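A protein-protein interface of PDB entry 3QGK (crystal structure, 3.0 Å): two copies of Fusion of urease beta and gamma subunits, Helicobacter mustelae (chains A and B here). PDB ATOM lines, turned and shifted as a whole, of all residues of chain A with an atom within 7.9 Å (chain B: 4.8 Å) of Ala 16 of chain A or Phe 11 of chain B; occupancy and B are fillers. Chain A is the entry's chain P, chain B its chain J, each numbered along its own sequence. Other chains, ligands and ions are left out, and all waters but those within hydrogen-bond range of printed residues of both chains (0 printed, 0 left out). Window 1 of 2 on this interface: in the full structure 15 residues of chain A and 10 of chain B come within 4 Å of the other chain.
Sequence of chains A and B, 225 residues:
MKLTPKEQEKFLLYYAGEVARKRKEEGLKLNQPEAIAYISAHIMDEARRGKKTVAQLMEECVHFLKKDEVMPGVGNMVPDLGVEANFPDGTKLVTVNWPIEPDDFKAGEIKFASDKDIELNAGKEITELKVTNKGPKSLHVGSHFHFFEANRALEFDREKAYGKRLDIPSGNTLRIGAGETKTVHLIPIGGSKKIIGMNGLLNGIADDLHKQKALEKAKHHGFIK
The side-chain hydroxyl of Tyr 14 of chain B sits at hydrogen-bond distance from the side-chain amino group of Lys 22 of chain A (2.7 Å).
OG of Ser 40 of chain A lies within hydrogen-bond range of O of Ile 36 of chain A (2.7 Å).
Among the printed residues, pairs that only touch across the chains: Tyr 15 of chain A with Tyr 15 of chain B, Tyr 15 of chain A with Tyr 14 of chain B, Pro 33 of chain A with FME 1 of chain B, Ala 16 of chain A with Phe 11 of chain B, Tyr 15 of chain A with Phe 11 of chain B, Leu 12 of chain A with Phe 11 of chain B, Ile 36 of chain A with FME 1 of chain B, Ala 16 of chain A with FME 1 of chain B and Ala 37 of chain A with FME 1 of chain B.
Of the printed residues of chain B, Leu 12 of chain A touches Phe 11 (3.7 Å). Of chain B, only FME 1 (3.9 Å) and Phe 11 (3.6 Å) come within 4 Å of Ala 16 of chain A. Of the printed residues of chain B, Pro 33 of chain A touches FME 1 (3.4 Å). Printed residues of chain A within 4 Å of Tyr 14 of chain B: Tyr 15 and Lys 22. The nearest printed residue of chain B that does not touch Ala 16 of chain A is Leu 3 of chain B (5.5 Å). The nearest printed residue of chain B that does not touch Lys 22 of chain A is Tyr 15 of chain B (9.0 Å).
Of the 24 printed residues of chain A, 7 touch a printed residue of chain B. Hydrophobic or aromatic side chains of chain A within 4 Å of the printed part of chain B: Leu 12, Tyr 15, Ala 16, Pro 33, Ile 36 and Ala 37. Of the 11 printed residues of chain B, 4 touch a printed residue of chain A. Hydrophobic or aromatic side chains of chain B within 4 Å of the printed part of chain A: Phe 11, Tyr 14 and Tyr 15. Among the printed residues, no Asp or Glu carboxylate lies within 4 Å of a Lys or Arg side-chain nitrogen of the other chain.
Leu 12 of chain A touches Phe 11 of chain B, but with the chains exchanged Phe 11 of chain A does not touch Leu 12 of chain B (9.7 Å). Tyr 15 of chain A touches Phe 11 of chain B, but with the chains exchanged Phe 11 of chain A does not touch Tyr 15 of chain B (8.6 Å). Tyr 15 of chain A touches Tyr 14 of chain B, but with the chains exchanged Tyr 14 of chain A does not touch Tyr 15 of chain B (9.3 Å). Tyr 15 of chain A touches its own counterpart, Tyr 15 of chain B. Positions printed for both chains: 9, 10, 11, 12, 13, 14 and 15.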
ATOM      1  N   GLU A   9      23.106  14.028   5.067  1.00  0.00           N
ATOM      2  CA  GLU A   9      22.909  12.595   4.795  1.00  0.00           C
ATOM      3  C   GLU A   9      21.685  12.102   5.549  1.00  0.00           C
ATOM      4  O   GLU A   9      20.811  11.472   4.955  1.00  0.00           O
ATOM      5  CB  GLU A   9      24.119  11.773   5.270  1.00  0.00           C
ATOM      6  CG  GLU A   9      25.347  11.818   4.376  1.00  0.00           C
ATOM      7  CD  GLU A   9      26.467  10.898   4.824  1.00  0.00           C
ATOM      8  OE1 GLU A   9      26.186   9.710   5.109  1.00  0.00           O
ATOM      9  OE2 GLU A   9      27.632  11.355   4.865  1.00  0.00           O
ATOM     10  N   LYS A  10      21.617  12.415   6.865  1.00  0.00           N
ATOM     11  CA  LYS A  10      20.530  12.008   7.763  1.00  0.00           C
ATOM     12  C   LYS A  10      19.154  12.508   7.326  1.00  0.00           C
ATOM     13  O   LYS A  10      18.175  11.787   7.516  1.00  0.00           O
ATOM     14  CB  LYS A  10      20.841  12.344   9.240  1.00  0.00           C
ATOM     15  CG  LYS A  10      22.122  11.703   9.809  1.00  0.00           C
ATOM     16  CD  LYS A  10      21.980  10.250  10.227  1.00  0.00           C
ATOM     17  CE  LYS A  10      23.333   9.683  10.605  1.00  0.00           C
ATOM     18  NZ  LYS A  10      23.313   8.200  10.774  1.00  0.00           N
ATOM     19  N   PHE A  11      19.080  13.703   6.690  1.00  0.00           N
ATOM     20  CA  PHE A  11      17.818  14.247   6.160  1.00  0.00           C
ATOM     21  C   PHE A  11      17.246  13.342   5.065  1.00  0.00           C
ATOM     22  O   PHE A  11      16.049  13.038   5.076  1.00  0.00           O
ATOM     23  CB  PHE A  11      17.990  15.684   5.648  1.00  0.00           C
ATOM     24  CG  PHE A  11      17.849  16.716   6.733  1.00  0.00           C
ATOM     25  CD1 PHE A  11      16.625  16.933   7.354  1.00  0.00           C
ATOM     26  CD2 PHE A  11      18.939  17.475   7.138  1.00  0.00           C
ATOM     27  CE1 PHE A  11      16.510  17.867   8.382  1.00  0.00           C
ATOM     28  CE2 PHE A  11      18.815  18.418   8.154  1.00  0.00           C
ATOM     29  CZ  PHE A  11      17.606  18.606   8.770  1.00  0.00           C
ATOM     30  N   LEU A  12      18.129  12.873   4.159  1.00  0.00           N
ATOM     31  CA  LEU A  12      17.783  11.952   3.074  1.00  0.00           C
ATOM     32  C   LEU A  12      17.299  10.624   3.657  1.00  0.00           C
ATOM     33  O   LEU A  12      16.241  10.133   3.248  1.00  0.00           O
ATOM     34  CB  LEU A  12      18.992  11.743   2.139  1.00  0.00           C
ATOM     35  CG  LEU A  12      18.883  10.663   1.070  1.00  0.00           C
ATOM     36  CD1 LEU A  12      17.857  11.034  -0.004  1.00  0.00           C
ATOM     37  CD2 LEU A  12      20.253  10.373   0.467  1.00  0.00           C
ATOM     38  N   LEU A  13      18.052  10.076   4.642  1.00  0.00           N
ATOM     39  CA  LEU A  13      17.677   8.842   5.320  1.00  0.00           C
ATOM     40  C   LEU A  13      16.321   9.002   5.965  1.00  0.00           C
ATOM     41  O   LEU A  13      15.473   8.138   5.778  1.00  0.00           O
ATOM     42  CB  LEU A  13      18.728   8.424   6.361  1.00  0.00           C
ATOM     43  CG  LEU A  13      18.407   7.179   7.197  1.00  0.00           C
ATOM     44  CD1 LEU A  13      18.352   5.933   6.349  1.00  0.00           C
ATOM     45  CD2 LEU A  13      19.410   7.016   8.312  1.00  0.00           C
ATOM     46  N   TYR A  14      16.106  10.119   6.686  1.00  0.00           N
ATOM     47  CA  TYR A  14      14.842  10.386   7.359  1.00  0.00           C
ATOM     48  C   TYR A  14      13.683  10.546   6.383  1.00  0.00           C
ATOM     49  O   TYR A  14      12.611   9.972   6.633  1.00  0.00           O
ATOM     50  CB  TYR A  14      14.931  11.556   8.358  1.00  0.00           C
ATOM     51  CG  TYR A  14      13.777  11.561   9.342  1.00  0.00           C
ATOM     52  CD1 TYR A  14      13.731  10.656  10.405  1.00  0.00           C
ATOM     53  CD2 TYR A  14      12.701  12.431   9.180  1.00  0.00           C
ATOM     54  CE1 TYR A  14      12.646  10.622  11.279  1.00  0.00           C
ATOM     55  CE2 TYR A  14      11.617  12.414  10.056  1.00  0.00           C
ATOM     56  CZ  TYR A  14      11.587  11.499  11.096  1.00  0.00           C
ATOM     57  OH  TYR A  14      10.515  11.495  11.952  1.00  0.00           O
ATOM     58  N   TYR A  15      13.901  11.266   5.251  1.00  0.00           N
ATOM     59  CA  TYR A  15      12.851  11.412   4.247  1.00  0.00           C
ATOM     60  C   TYR A  15      12.481  10.074   3.632  1.00  0.00           C
ATOM     61  O   TYR A  15      11.293   9.786   3.520  1.00  0.00           O
ATOM     62  CB  TYR A  15      13.174  12.454   3.180  1.00  0.00           C
ATOM     63  CG  TYR A  15      12.019  12.656   2.214  1.00  0.00           C
ATOM     64  CD1 TYR A  15      10.782  13.112   2.660  1.00  0.00           C
ATOM     65  CD2 TYR A  15      12.152  12.351   0.860  1.00  0.00           C
ATOM     66  CE1 TYR A  15       9.710  13.264   1.783  1.00  0.00           C
ATOM     67  CE2 TYR A  15      11.087  12.502  -0.026  1.00  0.00           C
ATOM     68  CZ  TYR A  15       9.865  12.952   0.442  1.00  0.00           C
ATOM     69  OH  TYR A  15       8.807  13.099  -0.421  1.00  0.00           O
ATOM     70  N   ALA A  16      13.495   9.230   3.304  1.00  0.00           N
ATOM     71  CA  ALA A  16      13.309   7.867   2.786  1.00  0.00           C
ATOM     72  C   ALA A  16      12.440   7.043   3.768  1.00  0.00           C
ATOM     73  O   ALA A  16      11.526   6.330   3.334  1.00  0.00           O
ATOM     74  CB  ALA A  16      14.651   7.190   2.581  1.00  0.00           C
ATOM     75  N   GLY A  17      12.679   7.227   5.071  1.00  0.00           N
ATOM     76  CA  GLY A  17      11.901   6.604   6.130  1.00  0.00           C
ATOM     77  C   GLY A  17      10.455   7.041   6.088  1.00  0.00           C
ATOM     78  O   GLY A  17       9.551   6.209   6.197  1.00  0.00           O
ATOM     79  N   GLU A  18      10.232   8.351   5.872  1.00  0.00           N
ATOM     80  CA  GLU A  18       8.895   8.937   5.779  1.00  0.00           C
ATOM     81  C   GLU A  18       8.133   8.426   4.545  1.00  0.00           C
ATOM     82  O   GLU A  18       6.952   8.084   4.674  1.00  0.00           O
ATOM     83  CB  GLU A  18       8.933  10.474   5.869  1.00  0.00           C
ATOM     84  CG  GLU A  18       9.402  10.984   7.226  1.00  0.00           C
ATOM     85  CD  GLU A  18       8.741  12.255   7.744  1.00  0.00           C
ATOM     86  OE1 GLU A  18       7.990  12.157   8.741  1.00  0.00           O
ATOM     87  OE2 GLU A  18       9.002  13.349   7.187  1.00  0.00           O
ATOM     88  N   VAL A  19       8.820   8.292   3.383  1.00  0.00           N
ATOM     89  CA  VAL A  19       8.228   7.741   2.147  1.00  0.00           C
ATOM     90  C   VAL A  19       7.832   6.278   2.386  1.00  0.00           C
ATOM     91  O   VAL A  19       6.720   5.878   2.017  1.00  0.00           O
ATOM     92  CB  VAL A  19       9.139   7.881   0.902  1.00  0.00           C
ATOM     93  CG1 VAL A  19       8.455   7.337  -0.351  1.00  0.00           C
ATOM     94  CG2 VAL A  19       9.534   9.331   0.680  1.00  0.00           C
ATOM     95  N   ALA A  20       8.730   5.494   3.035  1.00  0.00           N
ATOM     96  CA  ALA A  20       8.488   4.089   3.377  1.00  0.00           C
ATOM     97  C   ALA A  20       7.254   3.956   4.272  1.00  0.00           C
ATOM     98  O   ALA A  20       6.412   3.095   4.019  1.00  0.00           O
ATOM     99  CB  ALA A  20       9.706   3.497   4.061  1.00  0.00           C
ATOM    100  N   ARG A  21       7.120   4.847   5.276  1.00  0.00           N
ATOM    101  CA  ARG A  21       5.980   4.871   6.198  1.00  0.00           C
ATOM    102  C   ARG A  21       4.675   5.049   5.434  1.00  0.00           C
ATOM    103  O   ARG A  21       3.719   4.319   5.684  1.00  0.00           O
ATOM    104  CB  ARG A  21       6.144   5.986   7.244  1.00  0.00           C
ATOM    105  CG  ARG A  21       7.131   5.642   8.350  1.00  0.00           C
ATOM    106  CD  ARG A  21       7.637   6.865   9.081  1.00  0.00           C
ATOM    107  NE  ARG A  21       8.467   6.483  10.220  1.00  0.00           N
ATOM    108  CZ  ARG A  21       9.040   7.348  11.048  1.00  0.00           C
ATOM    109  NH1 ARG A  21       8.884   8.654  10.869  1.00  0.00           N
ATOM    110  NH2 ARG A  21       9.781   6.915  12.058  1.00  0.00           N
ATOM    111  N   LYS A  22       4.662   5.999   4.477  1.00  0.00           N
ATOM    112  CA  LYS A  22       3.521   6.328   3.621  1.00  0.00           C
ATOM    113  C   LYS A  22       3.087   5.098   2.815  1.00  0.00           C
ATOM    114  O   LYS A  22       1.904   4.767   2.804  1.00  0.00           O
ATOM    115  CB  LYS A  22       3.869   7.520   2.700  1.00  0.00           C
ATOM    116  CG  LYS A  22       2.701   8.018   1.852  1.00  0.00           C
ATOM    117  CD  LYS A  22       3.117   9.068   0.828  1.00  0.00           C
ATOM    118  CE  LYS A  22       2.107   9.125  -0.296  1.00  0.00           C
ATOM    119  NZ  LYS A  22       2.361  10.265  -1.208  1.00  0.00           N
ATOM    120  N   ARG A  23       4.056   4.406   2.195  1.00  0.00           N
ATOM    121  CA  ARG A  23       3.836   3.206   1.386  1.00  0.00           C
ATOM    122  C   ARG A  23       3.282   2.025   2.199  1.00  0.00           C
ATOM    123  O   ARG A  23       2.417   1.303   1.703  1.00  0.00           O
ATOM    124  CB  ARG A  23       5.116   2.840   0.617  1.00  0.00           C
ATOM    125  CG  ARG A  23       5.443   3.882  -0.441  1.00  0.00           C
ATOM    126  CD  ARG A  23       6.726   3.641  -1.196  1.00  0.00           C
ATOM    127  NE  ARG A  23       6.734   4.434  -2.427  1.00  0.00           N
ATOM    128  CZ  ARG A  23       7.750   4.501  -3.283  1.00  0.00           C
ATOM    129  NH1 ARG A  23       8.873   3.832  -3.048  1.00  0.00           N
ATOM    130  NH2 ARG A  23       7.644   5.223  -4.393  1.00  0.00           N
ATOM    131  N   LEU A  30       6.979  -3.538   1.835  1.00  0.00           N
ATOM    132  CA  LEU A  30       8.215  -2.794   1.659  1.00  0.00           C
ATOM    133  C   LEU A  30       9.354  -3.633   1.059  1.00  0.00           C
ATOM    134  O   LEU A  30       9.438  -4.835   1.315  1.00  0.00           O
ATOM    135  CB  LEU A  30       8.651  -2.153   2.986  1.00  0.00           C
ATOM    136  CG  LEU A  30       7.662  -1.212   3.693  1.00  0.00           C
ATOM    137  CD1 LEU A  30       8.243  -0.702   4.985  1.00  0.00           C
ATOM    138  CD2 LEU A  30       7.259  -0.038   2.816  1.00  0.00           C
ATOM    139  N   PRO A  33      15.528  -1.312   0.401  1.00  0.00           N
ATOM    140  CA  PRO A  33      15.822   0.044   0.896  1.00  0.00           C
ATOM    141  C   PRO A  33      14.707   0.694   1.720  1.00  0.00           C
ATOM    142  O   PRO A  33      15.007   1.420   2.677  1.00  0.00           O
ATOM    143  CB  PRO A  33      16.157   0.829  -0.374  1.00  0.00           C
ATOM    144  CG  PRO A  33      15.490   0.098  -1.455  1.00  0.00           C
ATOM    145  CD  PRO A  33      15.547  -1.347  -1.074  1.00  0.00           C
ATOM    146  N   GLU A  34      13.431   0.414   1.377  1.00  0.00           N
ATOM    147  CA  GLU A  34      12.278   0.954   2.103  1.00  0.00           C
ATOM    148  C   GLU A  34      12.278   0.441   3.539  1.00  0.00           C
ATOM    149  O   GLU A  34      12.149   1.246   4.463  1.00  0.00           O
ATOM    150  CB  GLU A  34      10.962   0.602   1.401  1.00  0.00           C
ATOM    151  CG  GLU A  34      10.702   1.373   0.116  1.00  0.00           C
ATOM    152  CD  GLU A  34       9.568   0.844  -0.749  1.00  0.00           C
ATOM    153  OE1 GLU A  34       9.011  -0.229  -0.420  1.00  0.00           O
ATOM    154  OE2 GLU A  34       9.237   1.499  -1.763  1.00  0.00           O
ATOM    155  N   ALA A  35      12.488  -0.885   3.725  1.00  0.00           N
ATOM    156  CA  ALA A  35      12.527  -1.542   5.033  1.00  0.00           C
ATOM    157  C   ALA A  35      13.619  -0.975   5.956  1.00  0.00           C
ATOM    158  O   ALA A  35      13.348  -0.680   7.128  1.00  0.00           O
ATOM    159  CB  ALA A  35      12.693  -3.044   4.864  1.00  0.00           C
ATOM    160  N   ILE A  36      14.830  -0.788   5.415  1.00  0.00           N
ATOM    161  CA  ILE A  36      15.975  -0.210   6.130  1.00  0.00           C
ATOM    162  C   ILE A  36      15.651   1.230   6.578  1.00  0.00           C
ATOM    163  O   ILE A  36      15.855   1.562   7.746  1.00  0.00           O
ATOM    164  CB  ILE A  36      17.257  -0.293   5.254  1.00  0.00           C
ATOM    165  CG1 ILE A  36      17.731  -1.743   5.111  1.00  0.00           C
ATOM    166  CG2 ILE A  36      18.354   0.558   5.825  1.00  0.00           C
ATOM    167  CD1 ILE A  36      18.491  -2.002   3.885  1.00  0.00           C
ATOM    168  N   ALA A  37      15.122   2.061   5.660  1.00  0.00           N
ATOM    169  CA  ALA A  37      14.758   3.441   5.946  1.00  0.00           C
ATOM    170  C   ALA A  37      13.622   3.543   6.966  1.00  0.00           C
ATOM    171  O   ALA A  37      13.661   4.425   7.829  1.00  0.00           O
ATOM    172  CB  ALA A  37      14.385   4.158   4.664  1.00  0.00           C
ATOM    173  N   TYR A  38      12.629   2.642   6.888  1.00  0.00           N
ATOM    174  CA  TYR A  38      11.505   2.619   7.822  1.00  0.00           C
ATOM    175  C   TYR A  38      12.001   2.411   9.267  1.00  0.00           C
ATOM    176  O   TYR A  38      11.585   3.143  10.179  1.00  0.00           O
ATOM    177  CB  TYR A  38      10.486   1.542   7.414  1.00  0.00           C
ATOM    178  CG  TYR A  38       9.307   1.396   8.359  1.00  0.00           C
ATOM    179  CD1 TYR A  38       8.164   2.175   8.207  1.00  0.00           C
ATOM    180  CD2 TYR A  38       9.310   0.433   9.364  1.00  0.00           C
ATOM    181  CE1 TYR A  38       7.059   2.011   9.043  1.00  0.00           C
ATOM    182  CE2 TYR A  38       8.215   0.264  10.211  1.00  0.00           C
ATOM    183  CZ  TYR A  38       7.090   1.052  10.044  1.00  0.00           C
ATOM    184  OH  TYR A  38       6.007   0.874  10.870  1.00  0.00           O
ATOM    185  N   SER A  40      15.244   2.733  10.332  1.00  0.00           N
ATOM    186  CA  SER A  40      16.186   3.824  10.622  1.00  0.00           C
ATOM    187  C   SER A  40      15.484   5.070  11.171  1.00  0.00           C
ATOM    188  O   SER A  40      15.901   5.585  12.208  1.00  0.00           O
ATOM    189  CB  SER A  40      17.017   4.165   9.393  1.00  0.00           C
ATOM    190  OG  SER A  40      17.790   3.038   9.019  1.00  0.00           O
ATOM    191  N   ALA A  41      14.387   5.508  10.514  1.00  0.00           N
ATOM    192  CA  ALA A  41      13.599   6.658  10.929  1.00  0.00           C
ATOM    193  C   ALA A  41      13.006   6.448  12.321  1.00  0.00           C
ATOM    194  O   ALA A  41      13.009   7.389  13.114  1.00  0.00           O
ATOM    195  CB  ALA A  41      12.516   6.949   9.912  1.00  0.00           C
ATOM    196  N   FME B   1      21.179   0.505   2.330  1.00  0.00           N
ATOM    197  CN  FME B   1      21.687  -0.724   2.351  1.00  0.00           C
ATOM    198  O1  FME B   1      22.500  -1.105   3.201  1.00  0.00           O
ATOM    199  CA  FME B   1      20.237   0.946   1.300  1.00  0.00           C
ATOM    200  CB  FME B   1      19.786   2.389   1.570  1.00  0.00           C
ATOM    201  CG  FME B   1      18.717   2.496   2.632  1.00  0.00           C
ATOM    202  SD  FME B   1      18.006   4.149   2.735  1.00  0.00           S
ATOM    203  CE  FME B   1      16.791   4.076   1.489  1.00  0.00           C
ATOM    204  C   FME B   1      20.825   0.855  -0.119  1.00  0.00           C
ATOM    205  O   FME B   1      20.107   0.508  -1.068  1.00  0.00           O
ATOM    206  N   LEU B   3      22.016   3.451  -2.081  1.00  0.00           N
ATOM    207  CA  LEU B   3      21.360   4.444  -2.938  1.00  0.00           C
ATOM    208  C   LEU B   3      22.232   4.948  -4.088  1.00  0.00           C
ATOM    209  O   LEU B   3      23.311   5.533  -3.892  1.00  0.00           O
ATOM    210  CB  LEU B   3      20.705   5.600  -2.150  1.00  0.00           C
ATOM    211  CG  LEU B   3      19.553   5.240  -1.206  1.00  0.00           C
ATOM    212  CD1 LEU B   3      19.237   6.389  -0.271  1.00  0.00           C
ATOM    213  CD2 LEU B   3      18.310   4.830  -1.977  1.00  0.00           C
ATOM    214  N   GLU B   7      18.671   7.434  -7.736  1.00  0.00           N
ATOM    215  CA  GLU B   7      17.683   7.291  -6.660  1.00  0.00           C
ATOM    216  C   GLU B   7      17.637   8.581  -5.819  1.00  0.00           C
ATOM    217  O   GLU B   7      16.552   9.029  -5.463  1.00  0.00           O
ATOM    218  CB  GLU B   7      17.958   6.043  -5.792  1.00  0.00           C
ATOM    219  CG  GLU B   7      17.251   4.777  -6.271  1.00  0.00           C
ATOM    220  CD  GLU B   7      17.539   3.510  -5.477  1.00  0.00           C
ATOM    221  OE1 GLU B   7      16.750   3.193  -4.556  1.00  0.00           O
ATOM    222  OE2 GLU B   7      18.536   2.816  -5.794  1.00  0.00           O
ATOM    223  N   GLN B   8      18.809   9.209  -5.573  1.00  0.00           N
ATOM    224  CA  GLN B   8      18.954  10.474  -4.830  1.00  0.00           C
ATOM    225  C   GLN B   8      18.217  11.636  -5.541  1.00  0.00           C
ATOM    226  O   GLN B   8      17.607  12.482  -4.875  1.00  0.00           O
ATOM    227  CB  GLN B   8      20.441  10.815  -4.610  1.00  0.00           C
ATOM    228  CG  GLN B   8      21.168   9.856  -3.650  1.00  0.00           C
ATOM    229  CD  GLN B   8      22.680   9.965  -3.705  1.00  0.00           C
ATOM    230  OE1 GLN B   8      23.381   9.020  -4.100  1.00  0.00           O
ATOM    231  NE2 GLN B   8      23.221  11.110  -3.286  1.00  0.00           N
ATOM    232  N   GLU B   9      18.254  11.642  -6.896  1.00  0.00           N
ATOM    233  CA  GLU B   9      17.568  12.608  -7.761  1.00  0.00           C
ATOM    234  C   GLU B   9      16.057  12.458  -7.579  1.00  0.00           C
ATOM    235  O   GLU B   9      15.364  13.453  -7.348  1.00  0.00           O
ATOM    236  CB  GLU B   9      17.886  12.331  -9.240  1.00  0.00           C
ATOM    237  CG  GLU B   9      19.233  12.824  -9.731  1.00  0.00           C
ATOM    238  CD  GLU B   9      19.453  12.633 -11.225  1.00  0.00           C
ATOM    239  OE1 GLU B   9      18.550  12.994 -12.017  1.00  0.00           O
ATOM    240  OE2 GLU B   9      20.545  12.146 -11.602  1.00  0.00           O
ATOM    241  N   LYS B  10      15.554  11.203  -7.678  1.00  0.00           N
ATOM    242  CA  LYS B  10      14.130  10.868  -7.566  1.00  0.00           C
ATOM    243  C   LYS B  10      13.504  11.268  -6.219  1.00  0.00           C
ATOM    244  O   LYS B  10      12.329  11.645  -6.200  1.00  0.00           O
ATOM    245  CB  LYS B  10      13.845   9.400  -7.931  1.00  0.00           C
ATOM    246  CG  LYS B  10      14.273   8.992  -9.345  1.00  0.00           C
ATOM    247  CD  LYS B  10      13.288   9.370 -10.434  1.00  0.00           C
ATOM    248  CE  LYS B  10      13.868   9.049 -11.796  1.00  0.00           C
ATOM    249  NZ  LYS B  10      13.054   9.631 -12.906  1.00  0.00           N
ATOM    250  N   PHE B  11      14.297  11.252  -5.115  1.00  0.00           N
ATOM    251  CA  PHE B  11      13.822  11.681  -3.798  1.00  0.00           C
ATOM    252  C   PHE B  11      13.461  13.157  -3.825  1.00  0.00           C
ATOM    253  O   PHE B  11      12.395  13.532  -3.328  1.00  0.00           O
ATOM    254  CB  PHE B  11      14.846  11.392  -2.700  1.00  0.00           C
ATOM    255  CG  PHE B  11      14.731  10.007  -2.125  1.00  0.00           C
ATOM    256  CD1 PHE B  11      13.645   9.653  -1.336  1.00  0.00           C
ATOM    257  CD2 PHE B  11      15.723   9.060  -2.345  1.00  0.00           C
ATOM    258  CE1 PHE B  11      13.537   8.365  -0.806  1.00  0.00           C
ATOM    259  CE2 PHE B  11      15.617   7.773  -1.813  1.00  0.00           C
ATOM    260  CZ  PHE B  11      14.523   7.431  -1.055  1.00  0.00           C
ATOM    261  N   LEU B  12      14.329  13.985  -4.459  1.00  0.00           N
ATOM    262  CA  LEU B  12      14.119  15.427  -4.626  1.00  0.00           C
ATOM    263  C   LEU B  12      12.874  15.668  -5.473  1.00  0.00           C
ATOM    264  O   LEU B  12      12.017  16.452  -5.066  1.00  0.00           O
ATOM    265  CB  LEU B  12      15.344  16.100  -5.251  1.00  0.00           C
ATOM    266  CG  LEU B  12      15.191  17.582  -5.622  1.00  0.00           C
ATOM    267  CD1 LEU B  12      14.996  18.472  -4.373  1.00  0.00           C
ATOM    268  CD2 LEU B  12      16.356  18.057  -6.481  1.00  0.00           C
ATOM    269  N   LEU B  13      12.756  14.959  -6.621  1.00  0.00           N
ATOM    270  CA  LEU B  13      11.584  15.062  -7.484  1.00  0.00           C
ATOM    271  C   LEU B  13      10.321  14.706  -6.703  1.00  0.00           C
ATOM    272  O   LEU B  13       9.345  15.455  -6.761  1.00  0.00           O
ATOM    273  CB  LEU B  13      11.725  14.179  -8.731  1.00  0.00           C
ATOM    274  CG  LEU B  13      10.508  14.145  -9.674  1.00  0.00           C
ATOM    275  CD1 LEU B  13      10.247  15.505 -10.312  1.00  0.00           C
ATOM    276  CD2 LEU B  13      10.666  13.064 -10.718  1.00  0.00           C
ATOM    277  N   TYR B  14      10.361  13.591  -5.942  1.00  0.00           N
ATOM    278  CA  TYR B  14       9.223  13.150  -5.142  1.00  0.00           C
ATOM    279  C   TYR B  14       8.870  14.135  -4.039  1.00  0.00           C
ATOM    280  O   TYR B  14       7.683  14.419  -3.853  1.00  0.00           O
ATOM    281  CB  TYR B  14       9.384  11.708  -4.619  1.00  0.00           C
ATOM    282  CG  TYR B  14       8.068  11.106  -4.166  1.00  0.00           C
ATOM    283  CD1 TYR B  14       7.132  10.648  -5.089  1.00  0.00           C
ATOM    284  CD2 TYR B  14       7.730  11.057  -2.819  1.00  0.00           C
ATOM    285  CE1 TYR B  14       5.900  10.144  -4.680  1.00  0.00           C
ATOM    286  CE2 TYR B  14       6.509  10.540  -2.395  1.00  0.00           C
ATOM    287  CZ  TYR B  14       5.591  10.091  -3.328  1.00  0.00           C
ATOM    288  OH  TYR B  14       4.380   9.601  -2.888  1.00  0.00           O
ATOM    289  N   TYR B  15       9.885  14.701  -3.347  1.00  0.00           N
ATOM    290  CA  TYR B  15       9.622  15.688  -2.306  1.00  0.00           C
ATOM    291  C   TYR B  15       8.986  16.948  -2.888  1.00  0.00           C
ATOM    292  O   TYR B  15       7.999  17.426  -2.324  1.00  0.00           O
ATOM    293  CB  TYR B  15      10.855  16.003  -1.450  1.00  0.00           C
ATOM    294  CG  TYR B  15      10.541  16.977  -0.337  1.00  0.00           C
ATOM    295  CD1 TYR B  15       9.600  16.667   0.643  1.00  0.00           C
ATOM    296  CD2 TYR B  15      11.138  18.237  -0.295  1.00  0.00           C
ATOM    297  CE1 TYR B  15       9.276  17.575   1.647  1.00  0.00           C
ATOM    298  CE2 TYR B  15      10.833  19.148   0.713  1.00  0.00           C
ATOM    299  CZ  TYR B  15       9.897  18.813   1.677  1.00  0.00           C
ATOM    300  OH  TYR B  15       9.577  19.710   2.664  1.00  0.00           O
